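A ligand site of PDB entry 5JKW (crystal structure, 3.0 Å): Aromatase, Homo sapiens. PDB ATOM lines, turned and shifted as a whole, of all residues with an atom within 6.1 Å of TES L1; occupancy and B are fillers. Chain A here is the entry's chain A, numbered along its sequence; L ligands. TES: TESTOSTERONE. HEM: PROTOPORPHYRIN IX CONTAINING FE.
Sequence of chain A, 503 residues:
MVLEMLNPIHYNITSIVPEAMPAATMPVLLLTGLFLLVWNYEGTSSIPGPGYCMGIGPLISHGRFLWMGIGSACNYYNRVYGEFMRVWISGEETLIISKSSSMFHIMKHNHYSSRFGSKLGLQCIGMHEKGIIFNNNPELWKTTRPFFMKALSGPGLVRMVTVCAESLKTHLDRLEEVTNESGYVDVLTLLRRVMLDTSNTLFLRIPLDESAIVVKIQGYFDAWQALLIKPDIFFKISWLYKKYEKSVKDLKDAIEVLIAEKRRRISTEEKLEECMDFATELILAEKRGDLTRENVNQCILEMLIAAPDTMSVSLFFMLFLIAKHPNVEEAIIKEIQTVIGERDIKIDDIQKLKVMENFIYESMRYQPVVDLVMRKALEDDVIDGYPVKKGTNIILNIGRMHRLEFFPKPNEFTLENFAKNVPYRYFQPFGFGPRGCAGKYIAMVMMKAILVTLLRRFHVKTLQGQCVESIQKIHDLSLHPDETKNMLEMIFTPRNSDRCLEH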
ATOM      1  N   ARG A 115      -5.070  23.718 -10.276  1.00  0.00           N
ATOM      2  CA  ARG A 115      -3.960  23.312  -9.407  1.00  0.00           C
ATOM      3  C   ARG A 115      -4.491  23.294  -7.961  1.00  0.00           C
ATOM      4  O   ARG A 115      -5.703  23.230  -7.746  1.00  0.00           O
ATOM      5  CB  ARG A 115      -2.784  24.285  -9.575  1.00  0.00           C
ATOM      6  CG  ARG A 115      -2.479  24.625 -11.018  1.00  0.00           C
ATOM      7  CD  ARG A 115      -1.061  25.113 -11.211  1.00  0.00           C
ATOM      8  NE  ARG A 115      -0.874  25.474 -12.620  1.00  0.00           N
ATOM      9  CZ  ARG A 115      -0.553  24.634 -13.599  1.00  0.00           C
ATOM     10  NH1 ARG A 115      -0.333  23.344 -13.381  1.00  0.00           N
ATOM     11  NH2 ARG A 115      -0.436  25.111 -14.837  1.00  0.00           N
ATOM     12  N   ILE A 133      -1.421  31.395 -12.861  1.00  0.00           N
ATOM     13  CA  ILE A 133      -0.544  30.243 -12.606  1.00  0.00           C
ATOM     14  C   ILE A 133      -1.162  29.342 -11.544  1.00  0.00           C
ATOM     15  O   ILE A 133      -1.278  28.152 -11.766  1.00  0.00           O
ATOM     16  CB  ILE A 133       0.886  30.628 -12.196  1.00  0.00           C
ATOM     17  CG1 ILE A 133       1.545  31.466 -13.291  1.00  0.00           C
ATOM     18  CG2 ILE A 133       1.726  29.372 -11.988  1.00  0.00           C
ATOM     19  CD1 ILE A 133       2.770  32.227 -12.810  1.00  0.00           C
ATOM     20  N   PHE A 134      -1.566  29.925 -10.406  1.00  0.00           N
ATOM     21  CA  PHE A 134      -2.274  29.165  -9.347  1.00  0.00           C
ATOM     22  C   PHE A 134      -3.704  29.697  -9.121  1.00  0.00           C
ATOM     23  O   PHE A 134      -4.253  29.622  -8.021  1.00  0.00           O
ATOM     24  CB  PHE A 134      -1.451  29.123  -8.044  1.00  0.00           C
ATOM     25  CG  PHE A 134      -0.460  27.989  -7.988  1.00  0.00           C
ATOM     26  CD1 PHE A 134       0.831  28.136  -8.487  1.00  0.00           C
ATOM     27  CD2 PHE A 134      -0.835  26.749  -7.474  1.00  0.00           C
ATOM     28  CE1 PHE A 134       1.728  27.065  -8.465  1.00  0.00           C
ATOM     29  CE2 PHE A 134       0.061  25.689  -7.442  1.00  0.00           C
ATOM     30  CZ  PHE A 134       1.356  25.853  -7.938  1.00  0.00           C
ATOM     31  N   PHE A 221       9.501  34.689  -5.412  1.00  0.00           N
ATOM     32  CA  PHE A 221       9.500  33.248  -5.657  1.00  0.00           C
ATOM     33  C   PHE A 221       9.756  32.443  -4.377  1.00  0.00           C
ATOM     34  O   PHE A 221       9.101  31.419  -4.153  1.00  0.00           O
ATOM     35  CB  PHE A 221      10.501  32.827  -6.746  1.00  0.00           C
ATOM     36  CG  PHE A 221      10.417  31.360  -7.104  1.00  0.00           C
ATOM     37  CD1 PHE A 221       9.565  30.926  -8.113  1.00  0.00           C
ATOM     38  CD2 PHE A 221      11.141  30.402  -6.380  1.00  0.00           C
ATOM     39  CE1 PHE A 221       9.464  29.578  -8.414  1.00  0.00           C
ATOM     40  CE2 PHE A 221      11.035  29.048  -6.675  1.00  0.00           C
ATOM     41  CZ  PHE A 221      10.185  28.633  -7.695  1.00  0.00           C
ATOM     42  N   TRP A 224       6.420  32.438  -2.466  1.00  0.00           N
ATOM     43  CA  TRP A 224       5.538  31.508  -3.171  1.00  0.00           C
ATOM     44  C   TRP A 224       5.918  30.074  -2.828  1.00  0.00           C
ATOM     45  O   TRP A 224       5.079  29.307  -2.373  1.00  0.00           O
ATOM     46  CB  TRP A 224       5.606  31.818  -4.679  1.00  0.00           C
ATOM     47  CG  TRP A 224       4.896  30.900  -5.657  1.00  0.00           C
ATOM     48  CD1 TRP A 224       3.982  29.925  -5.377  1.00  0.00           C
ATOM     49  CD2 TRP A 224       5.037  30.923  -7.069  1.00  0.00           C
ATOM     50  NE1 TRP A 224       3.566  29.329  -6.540  1.00  0.00           N
ATOM     51  CE2 TRP A 224       4.192  29.927  -7.595  1.00  0.00           C
ATOM     52  CE3 TRP A 224       5.807  31.695  -7.951  1.00  0.00           C
ATOM     53  CZ2 TRP A 224       4.112  29.674  -8.973  1.00  0.00           C
ATOM     54  CZ3 TRP A 224       5.715  31.444  -9.320  1.00  0.00           C
ATOM     55  CH2 TRP A 224       4.874  30.442  -9.819  1.00  0.00           C
ATOM     56  N   GLU A 302       2.667  38.313 -12.931  1.00  0.00           N
ATOM     57  CA  GLU A 302       2.956  36.923 -13.319  1.00  0.00           C
ATOM     58  C   GLU A 302       3.694  36.767 -14.638  1.00  0.00           C
ATOM     59  O   GLU A 302       4.495  35.846 -14.783  1.00  0.00           O
ATOM     60  CB  GLU A 302       1.678  36.074 -13.301  1.00  0.00           C
ATOM     61  CG  GLU A 302       1.274  35.678 -11.887  1.00  0.00           C
ATOM     62  CD  GLU A 302       0.057  34.767 -11.810  1.00  0.00           C
ATOM     63  OE1 GLU A 302      -0.408  34.292 -12.876  1.00  0.00           O
ATOM     64  OE2 GLU A 302      -0.440  34.507 -10.683  1.00  0.00           O
ATOM     65  N   ILE A 305       7.573  37.801 -13.908  1.00  0.00           N
ATOM     66  CA  ILE A 305       8.381  36.843 -13.158  1.00  0.00           C
ATOM     67  C   ILE A 305       8.686  35.549 -13.920  1.00  0.00           C
ATOM     68  O   ILE A 305       9.711  34.920 -13.680  1.00  0.00           O
ATOM     69  CB  ILE A 305       7.761  36.496 -11.780  1.00  0.00           C
ATOM     70  CG1 ILE A 305       6.486  35.656 -11.907  1.00  0.00           C
ATOM     71  CG2 ILE A 305       7.490  37.772 -10.997  1.00  0.00           C
ATOM     72  CD1 ILE A 305       5.903  35.263 -10.579  1.00  0.00           C
ATOM     73  N   ALA A 306       7.798  35.180 -14.845  1.00  0.00           N
ATOM     74  CA  ALA A 306       7.794  33.832 -15.421  1.00  0.00           C
ATOM     75  C   ALA A 306       9.158  33.374 -15.928  1.00  0.00           C
ATOM     76  O   ALA A 306       9.666  32.340 -15.500  1.00  0.00           O
ATOM     77  CB  ALA A 306       6.771  33.743 -16.553  1.00  0.00           C
ATOM     78  N   ALA A 307       9.726  34.160 -16.826  1.00  0.00           N
ATOM     79  CA  ALA A 307      10.988  33.803 -17.459  1.00  0.00           C
ATOM     80  C   ALA A 307      12.183  33.895 -16.487  1.00  0.00           C
ATOM     81  O   ALA A 307      12.930  32.926 -16.344  1.00  0.00           O
ATOM     82  CB  ALA A 307      11.205  34.635 -18.720  1.00  0.00           C
ATOM     83  N   ASP A 309      12.144  33.415 -13.408  1.00  0.00           N
ATOM     84  CA  ASP A 309      12.060  32.267 -12.517  1.00  0.00           C
ATOM     85  C   ASP A 309      12.583  31.022 -13.193  1.00  0.00           C
ATOM     86  O   ASP A 309      13.414  30.317 -12.632  1.00  0.00           O
ATOM     87  CB  ASP A 309      10.615  32.037 -12.032  1.00  0.00           C
ATOM     88  CG  ASP A 309      10.140  33.099 -11.051  1.00  0.00           C
ATOM     89  OD1 ASP A 309      10.929  33.551 -10.191  1.00  0.00           O
ATOM     90  OD2 ASP A 309       8.950  33.485 -11.113  1.00  0.00           O
ATOM     91  N   THR A 310      12.153  30.773 -14.418  1.00  0.00           N
ATOM     92  CA  THR A 310      12.312  29.459 -15.021  1.00  0.00           C
ATOM     93  C   THR A 310      13.340  29.358 -16.153  1.00  0.00           C
ATOM     94  O   THR A 310      14.109  28.402 -16.199  1.00  0.00           O
ATOM     95  CB  THR A 310      10.952  28.974 -15.527  1.00  0.00           C
ATOM     96  OG1 THR A 310      10.397  29.961 -16.418  1.00  0.00           O
ATOM     97  CG2 THR A 310      10.008  28.768 -14.340  1.00  0.00           C
ATOM     98  N   VAL A 370      11.508  22.520 -13.909  1.00  0.00           N
ATOM     99  CA  VAL A 370      10.099  22.274 -13.570  1.00  0.00           C
ATOM    100  C   VAL A 370       9.855  20.788 -13.730  1.00  0.00           C
ATOM    101  O   VAL A 370       9.380  20.320 -14.764  1.00  0.00           O
ATOM    102  CB  VAL A 370       9.140  23.095 -14.462  1.00  0.00           C
ATOM    103  CG1 VAL A 370       7.711  22.971 -13.956  1.00  0.00           C
ATOM    104  CG2 VAL A 370       9.556  24.555 -14.504  1.00  0.00           C
ATOM    105  N   LEU A 372       7.950  18.864 -11.682  1.00  0.00           N
ATOM    106  CA  LEU A 372       6.641  18.384 -11.253  1.00  0.00           C
ATOM    107  C   LEU A 372       5.550  19.429 -11.447  1.00  0.00           C
ATOM    108  O   LEU A 372       5.823  20.626 -11.484  1.00  0.00           O
ATOM    109  CB  LEU A 372       6.713  17.904  -9.814  1.00  0.00           C
ATOM    110  CG  LEU A 372       7.105  18.957  -8.782  1.00  0.00           C
ATOM    111  CD1 LEU A 372       5.897  19.609  -8.121  1.00  0.00           C
ATOM    112  CD2 LEU A 372       7.985  18.306  -7.734  1.00  0.00           C
ATOM    113  N   VAL A 373       4.316  18.941 -11.546  1.00  0.00           N
ATOM    114  CA  VAL A 373       3.147  19.728 -11.903  1.00  0.00           C
ATOM    115  C   VAL A 373       2.001  19.427 -10.959  1.00  0.00           C
ATOM    116  O   VAL A 373       1.676  18.262 -10.741  1.00  0.00           O
ATOM    117  CB  VAL A 373       2.650  19.379 -13.316  1.00  0.00           C
ATOM    118  CG1 VAL A 373       1.375  20.144 -13.656  1.00  0.00           C
ATOM    119  CG2 VAL A 373       3.747  19.646 -14.340  1.00  0.00           C
ATOM    120  N   MET A 374       1.362  20.466 -10.452  1.00  0.00           N
ATOM    121  CA  MET A 374       0.295  20.329  -9.483  1.00  0.00           C
ATOM    122  C   MET A 374      -1.046  20.542 -10.168  1.00  0.00           C
ATOM    123  O   MET A 374      -1.251  21.577 -10.808  1.00  0.00           O
ATOM    124  CB  MET A 374       0.498  21.328  -8.352  1.00  0.00           C
ATOM    125  CG  MET A 374       1.809  21.112  -7.613  1.00  0.00           C
ATOM    126  SD  MET A 374       2.106  22.367  -6.358  1.00  0.00           S
ATOM    127  CE  MET A 374       0.915  21.902  -5.124  1.00  0.00           C
ATOM    128  N   ARG A 375      -1.945  19.564 -10.051  1.00  0.00           N
ATOM    129  CA  ARG A 375      -3.290  19.644 -10.604  1.00  0.00           C
ATOM    130  C   ARG A 375      -4.335  19.215  -9.577  1.00  0.00           C
ATOM    131  O   ARG A 375      -4.010  18.740  -8.503  1.00  0.00           O
ATOM    132  CB  ARG A 375      -3.416  18.768 -11.842  1.00  0.00           C
ATOM    133  CG  ARG A 375      -2.430  19.101 -12.955  1.00  0.00           C
ATOM    134  CD  ARG A 375      -2.550  20.526 -13.470  1.00  0.00           C
ATOM    135  NE  ARG A 375      -2.151  20.643 -14.864  1.00  0.00           N
ATOM    136  CZ  ARG A 375      -2.912  20.333 -15.908  1.00  0.00           C
ATOM    137  NH1 ARG A 375      -4.153  19.872 -15.724  1.00  0.00           N
ATOM    138  NH2 ARG A 375      -2.451  20.485 -17.149  1.00  0.00           N
ATOM    139  N   LEU A 477       9.616  23.439  -4.806  1.00  0.00           N
ATOM    140  CA  LEU A 477       8.595  23.748  -5.816  1.00  0.00           C
ATOM    141  C   LEU A 477       9.145  23.490  -7.222  1.00  0.00           C
ATOM    142  O   LEU A 477       8.532  22.786  -8.020  1.00  0.00           O
ATOM    143  CB  LEU A 477       8.121  25.219  -5.723  1.00  0.00           C
ATOM    144  CG  LEU A 477       6.639  25.617  -5.878  1.00  0.00           C
ATOM    145  CD1 LEU A 477       6.544  26.975  -6.548  1.00  0.00           C
ATOM    146  CD2 LEU A 477       5.761  24.599  -6.602  1.00  0.00           C
ATOM    147  N   SER A 478      10.308  24.075  -7.493  1.00  0.00           N
ATOM    148  CA  SER A 478      11.082  23.775  -8.696  1.00  0.00           C
ATOM    149  C   SER A 478      12.393  23.111  -8.265  1.00  0.00           C
ATOM    150  O   SER A 478      12.627  22.895  -7.080  1.00  0.00           O
ATOM    151  CB  SER A 478      11.337  25.054  -9.499  1.00  0.00           C
ATOM    152  OG  SER A 478      12.098  25.998  -8.755  1.00  0.00           O
HETATM  153  C1  TES L   1       5.327  29.245 -13.770  1.00  0.00           C
HETATM  154  C2  TES L   1       6.126  30.498 -14.107  1.00  0.00           C
HETATM  155  C3  TES L   1       7.021  30.841 -12.956  1.00  0.00           C
HETATM  156  O3  TES L   1       7.248  32.013 -12.708  1.00  0.00           O
HETATM  157  C4  TES L   1       7.595  29.775 -12.113  1.00  0.00           C
HETATM  158  C5  TES L   1       7.239  28.488 -12.297  1.00  0.00           C
HETATM  159  C6  TES L   1       7.966  27.425 -11.501  1.00  0.00           C
HETATM  160  C7  TES L   1       6.976  26.528 -10.779  1.00  0.00           C
HETATM  161  C8  TES L   1       5.933  25.985 -11.744  1.00  0.00           C
HETATM  162  C9  TES L   1       5.196  27.135 -12.447  1.00  0.00           C
HETATM  163  C10 TES L   1       6.139  28.058 -13.252  1.00  0.00           C
HETATM  164  C11 TES L   1       3.977  26.624 -13.238  1.00  0.00           C
HETATM  165  C12 TES L   1       3.054  25.740 -12.412  1.00  0.00           C
HETATM  166  C13 TES L   1       3.807  24.580 -11.801  1.00  0.00           C
HETATM  167  C14 TES L   1       4.942  25.137 -10.961  1.00  0.00           C
HETATM  168  C15 TES L   1       5.436  23.932 -10.182  1.00  0.00           C
HETATM  169  C16 TES L   1       4.145  23.168  -9.860  1.00  0.00           C
HETATM  170  C17 TES L   1       3.052  23.847 -10.701  1.00  0.00           C
HETATM  171  O17 TES L   1       2.040  22.955 -11.163  1.00  0.00           O
HETATM  172  C18 TES L   1       4.267  23.595 -12.887  1.00  0.00           C
HETATM  173  C19 TES L   1       6.783  27.364 -14.444  1.00  0.00           C
HETATM  174  CHA HEM L   2       2.852  26.591 -16.656  1.00  0.00           C
HETATM  175  CHB HEM L   2       7.161  24.713 -17.745  1.00  0.00           C
HETATM  176  CHC HEM L   2       8.596  29.033 -19.377  1.00  0.00           C
HETATM  177  CHD HEM L   2       4.273  30.833 -18.434  1.00  0.00           C
HETATM  178  C1A HEM L   2       3.889  25.709 -16.850  1.00  0.00           C
HETATM  179  C2A HEM L   2       3.830  24.340 -16.541  1.00  0.00           C
HETATM  180  C3A HEM L   2       5.036  23.807 -16.842  1.00  0.00           C
HETATM  181  C4A HEM L   2       5.844  24.844 -17.351  1.00  0.00           C
HETATM  182  CMA HEM L   2       5.382  22.350 -16.653  1.00  0.00           C
HETATM  183  CAA HEM L   2       2.660  23.570 -15.988  1.00  0.00           C
HETATM  184  CBA HEM L   2       1.698  23.281 -17.149  1.00  0.00           C
HETATM  185  CGA HEM L   2       0.722  22.177 -16.787  1.00  0.00           C
HETATM  186  O1A HEM L   2       0.161  22.157 -15.673  1.00  0.00           O
HETATM  187  O2A HEM L   2       0.443  21.289 -17.615  1.00  0.00           O
HETATM  188  C1B HEM L   2       7.959  25.741 -18.255  1.00  0.00           C
HETATM  189  C2B HEM L   2       9.329  25.581 -18.626  1.00  0.00           C
HETATM  190  C3B HEM L   2       9.762  26.805 -19.099  1.00  0.00           C
HETATM  191  C4B HEM L   2       8.576  27.698 -18.979  1.00  0.00           C
HETATM  192  CMB HEM L   2      10.064  24.268 -18.497  1.00  0.00           C
HETATM  193  CAB HEM L   2      11.067  27.288 -19.636  1.00  0.00           C
HETATM  194  CBB HEM L   2      12.188  26.594 -19.779  1.00  0.00           C
HETATM  195  C1C HEM L   2       7.542  29.911 -19.305  1.00  0.00           C
HETATM  196  C2C HEM L   2       7.552  31.252 -19.753  1.00  0.00           C
HETATM  197  C3C HEM L   2       6.289  31.786 -19.489  1.00  0.00           C
HETATM  198  C4C HEM L   2       5.546  30.733 -18.875  1.00  0.00           C
HETATM  199  CMC HEM L   2       8.723  31.944 -20.410  1.00  0.00           C
HETATM  200  CAC HEM L   2       5.744  33.162 -19.736  1.00  0.00           C
HETATM  201  CBC HEM L   2       6.410  34.199 -20.264  1.00  0.00           C
HETATM  202  C1D HEM L   2       3.584  29.786 -17.854  1.00  0.00           C
HETATM  203  C2D HEM L   2       2.224  29.999 -17.364  1.00  0.00           C
HETATM  204  C3D HEM L   2       1.805  28.841 -16.878  1.00  0.00           C
HETATM  205  C4D HEM L   2       2.945  27.909 -17.052  1.00  0.00           C
HETATM  206  CMD HEM L   2       1.435  31.280 -17.420  1.00  0.00           C
HETATM  207  CAD HEM L   2       0.468  28.574 -16.232  1.00  0.00           C
HETATM  208  CBD HEM L   2      -0.588  28.078 -17.207  1.00  0.00           C
HETATM  209  CGD HEM L   2      -1.898  27.879 -16.477  1.00  0.00           C
HETATM  210  O1D HEM L   2      -2.961  28.128 -17.080  1.00  0.00           O
HETATM  211  O2D HEM L   2      -1.935  27.467 -15.294  1.00  0.00           O
HETATM  212  NA  HEM L   2       5.129  26.009 -17.360  1.00  0.00           N
HETATM  213  NB  HEM L   2       7.568  26.978 -18.500  1.00  0.00           N
HETATM  214  NC  HEM L   2       6.326  29.617 -18.789  1.00  0.00           N
HETATM  215  ND  HEM L   2       3.986  28.509 -17.670  1.00  0.00           N
HETATM  216 FE   HEM L   2       5.686  27.770 -18.083  1.00  0.00          FE
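The backbone NH of Met 374 is in hydrogen-bond range of an oxygen (O17) of TES L1 (2.7 Å).
An oxygen (O17) of TES L1 lies within hydrogen-bond range of the guanidinium group of Arg 115 (3.3 Å).
The guanidinium group (NH1) of Arg 115 lies within salt-bridge range of an oxygen (O1A) of HEM L2, at 2.6 Å.
NE of Arg 375 lies within salt-bridge range of O1A of HEM L2 (2.9 Å).
An oxygen (O3) of TES L1 sits close to the side-chain carboxylate (OD2) of Asp 309, 2.8 Å away.
Residues that only touch TES L1: Ala 306, Thr 310, Leu 372, Val 373, Trp 224, Leu 477, Val 370, Ile 133, Ile 305 and Phe 134.
Hydrophobic or aromatic side chains that line TES L1: Ile 133, Phe 134, Trp 224, Ile 305, Val 370, Val 373, Met 374 and Leu 477.
Of the 18 residues printed, 13 come within 4 Å of TES L1.
NH1 of Arg 115 sits at hydrogen-bond distance from O of Met 374 (3.3 Å).
The guanidinium group (NE) of Arg 115 is in hydrogen-bond range of the backbone carbonyl oxygen (O) of Ile 133 (2.8 Å).
The side-chain hydroxyl (OG1) of Thr 310 is in hydrogen-bond range of the backbone carbonyl oxygen (O) of Ala 306 (2.7 Å).
The backbone NH (N) of Ile 133 lies within hydrogen-bond range of the side-chain carboxylate (OE1) of Glu 302, at 3.1 Å.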
